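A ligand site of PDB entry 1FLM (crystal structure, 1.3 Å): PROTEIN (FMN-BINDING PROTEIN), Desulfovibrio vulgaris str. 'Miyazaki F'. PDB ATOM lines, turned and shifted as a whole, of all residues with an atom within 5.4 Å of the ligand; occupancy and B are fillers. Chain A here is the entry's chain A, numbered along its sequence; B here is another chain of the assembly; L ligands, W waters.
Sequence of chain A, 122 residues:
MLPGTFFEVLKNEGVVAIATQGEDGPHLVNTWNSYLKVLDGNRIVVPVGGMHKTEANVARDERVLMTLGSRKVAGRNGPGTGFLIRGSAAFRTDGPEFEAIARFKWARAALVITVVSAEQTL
Residues that only touch the ligand: Thr 121 of chain B (3.3 Å), Tyr 35 (3.4 Å), Val 29 (3.5 Å), Trp 32 (3.5 Å), Gly 82 of chain B (3.6 Å), Val 48 (3.7 Å), Leu 122 of chain B (3.8 Å) and Trp 106 (3.8 Å).
Hydrophobic or aromatic side chains within 4 Å of the ligand: His 27, Val 29, Trp 32, Tyr 35, Met 51, His 52, Trp 106 and Leu 122 of chain B.
Within 4 Å of the ligand: His 27, Val 29, Asn 30, Thr 31, Trp 32, Tyr 35, Pro 47, Val 48, Gly 49, Gly 50, Met 51, His 52, Lys 53, Thr 54, Trp 106, Gly 82 of chain B, Thr 121 of chain B and Leu 122 of chain B.
The nearest printed residue that does not touch the ligand is Val 15 (4.1 Å).
Water W3 lies within hydrogen-bond range of the side-chain amide oxygen of Asn 30, the side-chain hydroxyl of Thr 121 of chain B and an oxygen (O3) of the ligand.
Water W6 lies within hydrogen-bond range of O of Thr 121 of chain B and O4 of the ligand.
Water W1 lies within hydrogen-bond range of the backbone NH of Gly 50 (3.5 Å) and an oxygen (O1) of the ligand (3.5 Å).
The backbone NH of Thr 54 lies within hydrogen-bond range of an oxygen (O9) of the ligand (2.9 Å).
The side-chain hydroxyl of Thr 54 is in hydrogen-bond range of an oxygen (O9) of the ligand (2.7 Å).
A ring nitrogen (NE2) of His 27 sits at hydrogen-bond distance from an oxygen (O7) of the ligand, at 2.7 Å.
OG1 of Thr 31 lies within hydrogen-bond range of O2 of the ligand.
The backbone NH (N) of Gly 49 sits at hydrogen-bond distance from an oxygen (O1) of the ligand, 2.8 Å away.
The backbone NH (N) of Met 51 sits at hydrogen-bond distance from an oxygen (O5) of the ligand, 2.8 Å away.
N of Asn 30 sits at hydrogen-bond distance from O3 of the ligand (2.9 Å).
The backbone carbonyl oxygen (O) of Pro 47 is in hydrogen-bond range of a nitrogen (N2) of the ligand, 3.0 Å away.
O8 of the ligand sits at hydrogen-bond distance from N of His 52.
The backbone NH (N) of Lys 53 sits at hydrogen-bond distance from an oxygen (O8) of the ligand, 3.0 Å away.
An oxygen (O1) of the ligand sits at hydrogen-bond distance from the backbone NH of Gly 50 (3.0 Å).
N of Thr 121 of chain B lies within hydrogen-bond range of O of Gly 82 of chain B (3.0 Å).
The chain-end carboxylate (O) of Leu 122 of chain B lies within hydrogen-bond range of the side-chain hydroxyl (OG1) of Thr 81 of chain B (2.7 Å).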
ATOM      1  N   VAL A  15     -29.176 -16.743 -12.164  1.00  0.00           N
ATOM      2  CA  VAL A  15     -28.389 -15.846 -11.315  1.00  0.00           C
ATOM      3  C   VAL A  15     -27.767 -16.664 -10.183  1.00  0.00           C
ATOM      4  O   VAL A  15     -28.489 -17.331  -9.404  1.00  0.00           O
ATOM      5  CB  VAL A  15     -29.285 -14.730 -10.712  1.00  0.00           C
ATOM      6  CG1 VAL A  15     -28.450 -13.866  -9.783  1.00  0.00           C
ATOM      7  CG2 VAL A  15     -29.830 -13.908 -11.862  1.00  0.00           C
ATOM      8  N   HIS A  27     -21.733 -10.220   2.886  1.00  0.00           N
ATOM      9  CA  HIS A  27     -21.802  -9.519   1.633  1.00  0.00           C
ATOM     10  C   HIS A  27     -22.305 -10.534   0.582  1.00  0.00           C
ATOM     11  O   HIS A  27     -22.114 -11.725   0.787  1.00  0.00           O
ATOM     12  CB  HIS A  27     -20.450  -8.919   1.234  1.00  0.00           C
ATOM     13  CG  HIS A  27     -20.537  -8.041   0.038  1.00  0.00           C
ATOM     14  ND1 HIS A  27     -21.591  -7.115  -0.057  1.00  0.00           N
ATOM     15  CD2 HIS A  27     -19.774  -7.914  -1.066  1.00  0.00           C
ATOM     16  CE1 HIS A  27     -21.440  -6.440  -1.209  1.00  0.00           C
ATOM     17  NE2 HIS A  27     -20.364  -6.916  -1.834  1.00  0.00           N
ATOM     18  N   VAL A  29     -22.761 -11.134  -3.718  1.00  0.00           N
ATOM     19  CA  VAL A  29     -22.569 -10.692  -5.105  1.00  0.00           C
ATOM     20  C   VAL A  29     -23.019 -11.807  -6.028  1.00  0.00           C
ATOM     21  O   VAL A  29     -23.407 -12.915  -5.592  1.00  0.00           O
ATOM     22  CB  VAL A  29     -21.097 -10.343  -5.386  1.00  0.00           C
ATOM     23  CG1 VAL A  29     -20.642  -9.160  -4.506  1.00  0.00           C
ATOM     24  CG2 VAL A  29     -20.155 -11.529  -5.211  1.00  0.00           C
ATOM     25  N   ASN A  30     -23.025 -11.557  -7.313  1.00  0.00           N
ATOM     26  CA  ASN A  30     -23.593 -12.475  -8.286  1.00  0.00           C
ATOM     27  C   ASN A  30     -22.672 -12.725  -9.464  1.00  0.00           C
ATOM     28  O   ASN A  30     -21.753 -12.013  -9.817  1.00  0.00           O
ATOM     29  CB  ASN A  30     -24.875 -11.865  -8.880  1.00  0.00           C
ATOM     30  CG  ASN A  30     -25.890 -11.626  -7.806  1.00  0.00           C
ATOM     31  OD1 ASN A  30     -26.221 -10.442  -7.531  1.00  0.00           O
ATOM     32  ND2 ASN A  30     -26.436 -12.628  -7.136  1.00  0.00           N
ATOM     33  N   THR A  31     -23.017 -13.843 -10.142  1.00  0.00           N
ATOM     34  CA  THR A  31     -22.572 -14.106 -11.508  1.00  0.00           C
ATOM     35  C   THR A  31     -23.708 -14.852 -12.200  1.00  0.00           C
ATOM     36  O   THR A  31     -24.830 -14.877 -11.663  1.00  0.00           O
ATOM     37  CB  THR A  31     -21.206 -14.817 -11.523  1.00  0.00           C
ATOM     38  OG1 THR A  31     -20.732 -14.909 -12.876  1.00  0.00           O
ATOM     39  CG2 THR A  31     -21.320 -16.239 -10.990  1.00  0.00           C
ATOM     40  N   TRP A  32     -23.460 -15.363 -13.397  1.00  0.00           N
ATOM     41  CA  TRP A  32     -24.473 -16.043 -14.183  1.00  0.00           C
ATOM     42  C   TRP A  32     -24.152 -17.543 -14.236  1.00  0.00           C
ATOM     43  O   TRP A  32     -22.945 -17.872 -14.311  1.00  0.00           O
ATOM     44  CB  TRP A  32     -24.536 -15.535 -15.622  1.00  0.00           C
ATOM     45  CG  TRP A  32     -24.884 -14.084 -15.785  1.00  0.00           C
ATOM     46  CD1 TRP A  32     -24.002 -13.073 -16.057  1.00  0.00           C
ATOM     47  CD2 TRP A  32     -26.205 -13.525 -15.736  1.00  0.00           C
ATOM     48  NE1 TRP A  32     -24.732 -11.897 -16.146  1.00  0.00           N
ATOM     49  CE2 TRP A  32     -26.044 -12.132 -15.964  1.00  0.00           C
ATOM     50  CE3 TRP A  32     -27.474 -14.045 -15.519  1.00  0.00           C
ATOM     51  CZ2 TRP A  32     -27.138 -11.237 -15.989  1.00  0.00           C
ATOM     52  CZ3 TRP A  32     -28.553 -13.126 -15.538  1.00  0.00           C
ATOM     53  CH2 TRP A  32     -28.375 -11.750 -15.768  1.00  0.00           C
ATOM     54  N   TYR A  35     -21.638 -18.430 -16.875  1.00  0.00           N
ATOM     55  CA  TYR A  35     -20.253 -17.991 -16.740  1.00  0.00           C
ATOM     56  C   TYR A  35     -19.426 -18.965 -15.906  1.00  0.00           C
ATOM     57  O   TYR A  35     -18.183 -18.841 -15.943  1.00  0.00           O
ATOM     58  CB  TYR A  35     -20.197 -16.594 -16.066  1.00  0.00           C
ATOM     59  CG  TYR A  35     -20.554 -15.372 -16.907  1.00  0.00           C
ATOM     60  CD1 TYR A  35     -21.189 -15.487 -18.109  1.00  0.00           C
ATOM     61  CD2 TYR A  35     -20.235 -14.103 -16.390  1.00  0.00           C
ATOM     62  CE1 TYR A  35     -21.503 -14.318 -18.849  1.00  0.00           C
ATOM     63  CE2 TYR A  35     -20.530 -12.965 -17.086  1.00  0.00           C
ATOM     64  CZ  TYR A  35     -21.151 -13.100 -18.303  1.00  0.00           C
ATOM     65  OH  TYR A  35     -21.473 -11.962 -19.036  1.00  0.00           O
ATOM     66  N   VAL A  46     -15.094 -18.490 -11.370  1.00  0.00           N
ATOM     67  CA  VAL A  46     -15.997 -17.362 -11.682  1.00  0.00           C
ATOM     68  C   VAL A  46     -15.135 -16.258 -12.279  1.00  0.00           C
ATOM     69  O   VAL A  46     -14.105 -15.931 -11.662  1.00  0.00           O
ATOM     70  CB  VAL A  46     -16.645 -16.861 -10.398  1.00  0.00           C
ATOM     71  CG1 VAL A  46     -17.510 -15.606 -10.646  1.00  0.00           C
ATOM     72  CG2 VAL A  46     -17.476 -18.006  -9.751  1.00  0.00           C
ATOM     73  N   PRO A  47     -15.543 -15.616 -13.357  1.00  0.00           N
ATOM     74  CA  PRO A  47     -14.769 -14.457 -13.853  1.00  0.00           C
ATOM     75  C   PRO A  47     -15.059 -13.223 -13.008  1.00  0.00           C
ATOM     76  O   PRO A  47     -16.230 -12.847 -12.756  1.00  0.00           O
ATOM     77  CB  PRO A  47     -15.274 -14.357 -15.304  1.00  0.00           C
ATOM     78  CG  PRO A  47     -16.696 -14.863 -15.244  1.00  0.00           C
ATOM     79  CD  PRO A  47     -16.717 -15.929 -14.149  1.00  0.00           C
ATOM     80  N   VAL A  48     -14.007 -12.581 -12.549  1.00  0.00           N
ATOM     81  CA  VAL A  48     -14.100 -11.417 -11.670  1.00  0.00           C
ATOM     82  C   VAL A  48     -13.832 -10.147 -12.472  1.00  0.00           C
ATOM     83  O   VAL A  48     -12.740  -9.956 -13.036  1.00  0.00           O
ATOM     84  CB  VAL A  48     -13.031 -11.511 -10.559  1.00  0.00           C
ATOM     85  CG1 VAL A  48     -13.074 -10.258  -9.710  1.00  0.00           C
ATOM     86  CG2 VAL A  48     -13.236 -12.773  -9.703  1.00  0.00           C
ATOM     87  N   GLY A  49     -14.813  -9.269 -12.484  1.00  0.00           N
ATOM     88  CA  GLY A  49     -14.608  -7.912 -13.027  1.00  0.00           C
ATOM     89  C   GLY A  49     -14.545  -6.934 -11.886  1.00  0.00           C
ATOM     90  O   GLY A  49     -13.609  -6.147 -11.769  1.00  0.00           O
ATOM     91  N   GLY A  50     -15.517  -6.951 -10.991  1.00  0.00           N
ATOM     92  CA  GLY A  50     -15.523  -6.106  -9.807  1.00  0.00           C
ATOM     93  C   GLY A  50     -15.140  -6.912  -8.595  1.00  0.00           C
ATOM     94  O   GLY A  50     -13.935  -7.232  -8.492  1.00  0.00           O
ATOM     95  N   MET A  51     -16.057  -7.270  -7.726  1.00  0.00           N
ATOM     96  CA  MET A  51     -15.793  -8.104  -6.541  1.00  0.00           C
ATOM     97  C   MET A  51     -14.618  -7.592  -5.716  1.00  0.00           C
ATOM     98  O   MET A  51     -13.808  -8.326  -5.196  1.00  0.00           O
ATOM     99  CB  MET A  51     -15.603  -9.585  -6.931  1.00  0.00           C
ATOM    100  CG  MET A  51     -16.890 -10.081  -7.589  1.00  0.00           C
ATOM    101  SD  MET A  51     -16.807 -11.894  -7.718  1.00  0.00           S
ATOM    102  CE  MET A  51     -18.357 -12.265  -8.534  1.00  0.00           C
ATOM    103  N   HIS A  52     -14.576  -6.262  -5.544  1.00  0.00           N
ATOM    104  CA  HIS A  52     -13.532  -5.692  -4.696  1.00  0.00           C
ATOM    105  C   HIS A  52     -13.828  -5.871  -3.240  1.00  0.00           C
ATOM    106  O   HIS A  52     -12.962  -6.205  -2.445  1.00  0.00           O
ATOM    107  CB  HIS A  52     -13.369  -4.175  -5.013  1.00  0.00           C
ATOM    108  CG  HIS A  52     -12.910  -4.012  -6.442  1.00  0.00           C
ATOM    109  ND1 HIS A  52     -11.619  -4.236  -6.846  1.00  0.00           N
ATOM    110  CD2 HIS A  52     -13.576  -3.651  -7.550  1.00  0.00           C
ATOM    111  CE1 HIS A  52     -11.498  -4.026  -8.156  1.00  0.00           C
ATOM    112  NE2 HIS A  52     -12.691  -3.678  -8.590  1.00  0.00           N
ATOM    113  N   LYS A  53     -15.065  -5.663  -2.796  1.00  0.00           N
ATOM    114  CA  LYS A  53     -15.364  -5.897  -1.375  1.00  0.00           C
ATOM    115  C   LYS A  53     -15.297  -7.380  -1.075  1.00  0.00           C
ATOM    116  O   LYS A  53     -14.838  -7.840  -0.028  1.00  0.00           O
ATOM    117  CB  LYS A  53     -16.764  -5.333  -1.040  1.00  0.00           C
ATOM    118  CG  LYS A  53     -17.181  -5.454   0.422  1.00  0.00           C
ATOM    119  CD  LYS A  53     -18.489  -4.672   0.601  1.00  0.00           C
ATOM    120  CE  LYS A  53     -18.679  -4.266   2.052  1.00  0.00           C
ATOM    121  NZ  LYS A  53     -18.296  -5.348   2.996  1.00  0.00           N
ATOM    122  N   THR A  54     -15.789  -8.200  -2.043  1.00  0.00           N
ATOM    123  CA  THR A  54     -15.702  -9.643  -1.890  1.00  0.00           C
ATOM    124  C   THR A  54     -14.238 -10.070  -1.744  1.00  0.00           C
ATOM    125  O   THR A  54     -14.002 -10.921  -0.854  1.00  0.00           O
ATOM    126  CB  THR A  54     -16.341 -10.257  -3.148  1.00  0.00           C
ATOM    127  OG1 THR A  54     -17.757  -9.907  -3.146  1.00  0.00           O
ATOM    128  CG2 THR A  54     -16.299 -11.774  -3.119  1.00  0.00           C
ATOM    129  N   GLU A  55     -13.360  -9.520  -2.566  1.00  0.00           N
ATOM    130  CA  GLU A  55     -11.944  -9.888  -2.444  1.00  0.00           C
ATOM    131  C   GLU A  55     -11.387  -9.524  -1.081  1.00  0.00           C
ATOM    132  O   GLU A  55     -10.659 -10.303  -0.445  1.00  0.00           O
ATOM    133  CB  GLU A  55     -11.149  -9.221  -3.546  1.00  0.00           C
ATOM    134  CG  GLU A  55      -9.685  -9.712  -3.523  1.00  0.00           C
ATOM    135  CD  GLU A  55      -8.904  -9.222  -4.709  1.00  0.00           C
ATOM    136  OE1 GLU A  55      -9.342  -8.370  -5.500  1.00  0.00           O
ATOM    137  OE2 GLU A  55      -7.749  -9.724  -4.867  1.00  0.00           O
ATOM    138  N   TRP A 106     -12.892  -8.500 -19.843  1.00  0.00           N
ATOM    139  CA  TRP A 106     -13.075  -7.595 -18.727  1.00  0.00           C
ATOM    140  C   TRP A 106     -12.628  -8.200 -17.381  1.00  0.00           C
ATOM    141  O   TRP A 106     -12.673  -7.474 -16.374  1.00  0.00           O
ATOM    142  CB  TRP A 106     -14.551  -7.217 -18.643  1.00  0.00           C
ATOM    143  CG  TRP A 106     -15.531  -8.330 -18.758  1.00  0.00           C
ATOM    144  CD1 TRP A 106     -16.210  -8.724 -19.892  1.00  0.00           C
ATOM    145  CD2 TRP A 106     -15.994  -9.222 -17.699  1.00  0.00           C
ATOM    146  NE1 TRP A 106     -17.053  -9.788 -19.622  1.00  0.00           N
ATOM    147  CE2 TRP A 106     -16.921 -10.099 -18.283  1.00  0.00           C
ATOM    148  CE3 TRP A 106     -15.688  -9.332 -16.350  1.00  0.00           C
ATOM    149  CZ2 TRP A 106     -17.568 -11.094 -17.554  1.00  0.00           C
ATOM    150  CZ3 TRP A 106     -16.335 -10.327 -15.621  1.00  0.00           C
ATOM    151  CH2 TRP A 106     -17.260 -11.194 -16.215  1.00  0.00           C
ATOM    152  N   LEU B  68     -31.353 -10.692  -6.904  1.00  0.00           N
ATOM    153  CA  LEU B  68     -32.251 -11.330  -7.890  1.00  0.00           C
ATOM    154  C   LEU B  68     -31.924 -10.672  -9.243  1.00  0.00           C
ATOM    155  O   LEU B  68     -31.299  -9.587  -9.298  1.00  0.00           O
ATOM    156  CB  LEU B  68     -33.706 -11.216  -7.536  1.00  0.00           C
ATOM    157  CG  LEU B  68     -34.346  -9.832  -7.680  1.00  0.00           C
ATOM    158  CD1 LEU B  68     -35.869  -9.950  -7.820  1.00  0.00           C
ATOM    159  CD2 LEU B  68     -33.972  -8.951  -6.492  1.00  0.00           C
ATOM    160  N   GLY B  69     -32.223 -11.293 -10.349  1.00  0.00           N
ATOM    161  CA  GLY B  69     -31.951 -10.681 -11.639  1.00  0.00           C
ATOM    162  C   GLY B  69     -32.604 -11.497 -12.746  1.00  0.00           C
ATOM    163  O   GLY B  69     -33.393 -12.419 -12.495  1.00  0.00           O
ATOM    164  N   THR B  81     -29.599  -8.043 -16.099  1.00  0.00           N
ATOM    165  CA  THR B  81     -29.329  -7.117 -14.976  1.00  0.00           C
ATOM    166  C   THR B  81     -29.796  -7.760 -13.695  1.00  0.00           C
ATOM    167  O   THR B  81     -30.378  -8.876 -13.730  1.00  0.00           O
ATOM    168  CB  THR B  81     -30.080  -5.772 -15.176  1.00  0.00           C
ATOM    169  OG1 THR B  81     -29.599  -4.828 -14.181  1.00  0.00           O
ATOM    170  CG2 THR B  81     -31.569  -5.854 -14.951  1.00  0.00           C
ATOM    171  N   GLY B  82     -29.582  -7.073 -12.588  1.00  0.00           N
ATOM    172  CA  GLY B  82     -30.099  -7.562 -11.311  1.00  0.00           C
ATOM    173  C   GLY B  82     -29.821  -6.516 -10.218  1.00  0.00           C
ATOM    174  O   GLY B  82     -29.267  -5.443 -10.535  1.00  0.00           O
ATOM    175  N   PHE B  83     -30.196  -6.871  -9.015  1.00  0.00           N
ATOM    176  CA  PHE B  83     -30.207  -5.933  -7.912  1.00  0.00           C
ATOM    177  C   PHE B  83     -29.629  -6.509  -6.635  1.00  0.00           C
ATOM    178  O   PHE B  83     -29.818  -7.719  -6.378  1.00  0.00           O
ATOM    179  CB  PHE B  83     -31.666  -5.531  -7.539  1.00  0.00           C
ATOM    180  CG  PHE B  83     -32.219  -4.600  -8.614  1.00  0.00           C
ATOM    181  CD1 PHE B  83     -32.791  -5.117  -9.759  1.00  0.00           C
ATOM    182  CD2 PHE B  83     -32.122  -3.230  -8.369  1.00  0.00           C
ATOM    183  CE1 PHE B  83     -33.220  -4.215 -10.771  1.00  0.00           C
ATOM    184  CE2 PHE B  83     -32.543  -2.368  -9.376  1.00  0.00           C
ATOM    185  CZ  PHE B  83     -33.093  -2.858 -10.510  1.00  0.00           C
ATOM    186  N   THR B 121     -26.943  -3.623 -10.003  1.00  0.00           N
ATOM    187  CA  THR B 121     -25.503  -3.815 -10.016  1.00  0.00           C
ATOM    188  C   THR B 121     -24.993  -4.267 -11.348  1.00  0.00           C
ATOM    189  O   THR B 121     -23.797  -4.654 -11.463  1.00  0.00           O
ATOM    190  CB  THR B 121     -25.122  -4.884  -8.939  1.00  0.00           C
ATOM    191  OG1 THR B 121     -25.968  -6.004  -9.177  1.00  0.00           O
ATOM    192  CG2 THR B 121     -25.327  -4.341  -7.529  1.00  0.00           C
ATOM    193  N   LEU B 122     -25.769  -4.244 -12.432  1.00  0.00           N
ATOM    194  CA  LEU B 122     -25.301  -4.491 -13.787  1.00  0.00           C
ATOM    195  C   LEU B 122     -26.127  -3.655 -14.754  1.00  0.00           C
ATOM    196  O   LEU B 122     -27.328  -3.471 -14.506  1.00  0.00           O
ATOM    197  CB  LEU B 122     -25.473  -6.008 -14.014  1.00  0.00           C
ATOM    198  CG  LEU B 122     -24.848  -6.735 -15.162  1.00  0.00           C
ATOM    199  CD1 LEU B 122     -23.335  -6.522 -15.073  1.00  0.00           C
ATOM    200  CD2 LEU B 122     -25.252  -8.217 -15.115  1.00  0.00           C
ATOM    201  OXT LEU B 122     -25.535  -3.247 -15.779  1.00  0.00           O
HETATM  202  N1  LIG L   1     -19.462  -9.084 -11.106  1.00  0.00           N
HETATM  203  C1  LIG L   1     -18.343  -9.703 -11.517  1.00  0.00           C
HETATM  204  O1  LIG L   1     -17.246  -9.440 -11.136  1.00  0.00           O
HETATM  205  N2  LIG L   1     -18.428 -10.883 -12.309  1.00  0.00           N
HETATM  206  C2  LIG L   1     -19.581 -11.414 -12.785  1.00  0.00           C
HETATM  207  O2  LIG L   1     -19.584 -12.464 -13.467  1.00  0.00           O
HETATM  208  C3  LIG L   1     -20.793 -10.699 -12.444  1.00  0.00           C
HETATM  209  N3  LIG L   1     -21.939 -11.148 -12.839  1.00  0.00           N
HETATM  210  C4  LIG L   1     -23.062 -10.553 -12.362  1.00  0.00           C
HETATM  211  C5  LIG L   1     -24.336 -11.114 -12.698  1.00  0.00           C
HETATM  212  C6  LIG L   1     -25.488 -10.585 -12.201  1.00  0.00           C
HETATM  213  C7  LIG L   1     -26.893 -11.126 -12.492  1.00  0.00           C
HETATM  214  C8  LIG L   1     -25.457  -9.332 -11.495  1.00  0.00           C
HETATM  215  C9  LIG L   1     -26.751  -8.708 -10.992  1.00  0.00           C
HETATM  216  C10 LIG L   1     -24.253  -8.790 -11.104  1.00  0.00           C
HETATM  217  C11 LIG L   1     -23.050  -9.391 -11.507  1.00  0.00           C
HETATM  218  N4  LIG L   1     -21.789  -8.922 -11.143  1.00  0.00           N
HETATM  219  C12 LIG L   1     -20.646  -9.527 -11.565  1.00  0.00           C
HETATM  220  C13 LIG L   1     -21.642  -7.729 -10.253  1.00  0.00           C
HETATM  221  C14 LIG L   1     -21.372  -8.292  -8.853  1.00  0.00           C
HETATM  222  O3  LIG L   1     -22.572  -8.880  -8.353  1.00  0.00           O
HETATM  223  C15 LIG L   1     -20.908  -7.198  -7.856  1.00  0.00           C
HETATM  224  O4  LIG L   1     -22.008  -6.182  -7.795  1.00  0.00           O
HETATM  225  C16 LIG L   1     -19.700  -6.450  -8.318  1.00  0.00           C
HETATM  226  O5  LIG L   1     -18.681  -7.343  -8.802  1.00  0.00           O
HETATM  227  C17 LIG L   1     -19.056  -5.662  -7.182  1.00  0.00           C
HETATM  228  O6  LIG L   1     -18.610  -6.579  -6.151  1.00  0.00           O
HETATM  229  P1  LIG L   1     -18.256  -6.113  -4.690  1.00  0.00           P
HETATM  230  O7  LIG L   1     -19.521  -5.563  -4.072  1.00  0.00           O
HETATM  231  O8  LIG L   1     -17.181  -4.998  -4.829  1.00  0.00           O
HETATM  232  O9  LIG L   1     -17.733  -7.366  -3.977  1.00  0.00           O
HETATM  233  O   HOH W   1     -17.928  -6.950 -13.487  1.00  0.00           O
HETATM  234  O   HOH W   2     -19.900  -3.434  -2.849  1.00  0.00           O
HETATM  235  O   HOH W   3     -25.119  -8.015  -7.551  1.00  0.00           O
HETATM  236  O   HOH W   4     -22.032  -5.375  -5.137  1.00  0.00           O
HETATM  237  O   HOH W   5     -19.001  -5.425 -11.618  1.00  0.00           O
HETATM  238  O   HOH W   6     -21.877  -3.877  -9.864  1.00  0.00           O
HETATM  239  O   HOH W   7     -19.920  -8.840 -14.815  1.00  0.00           O
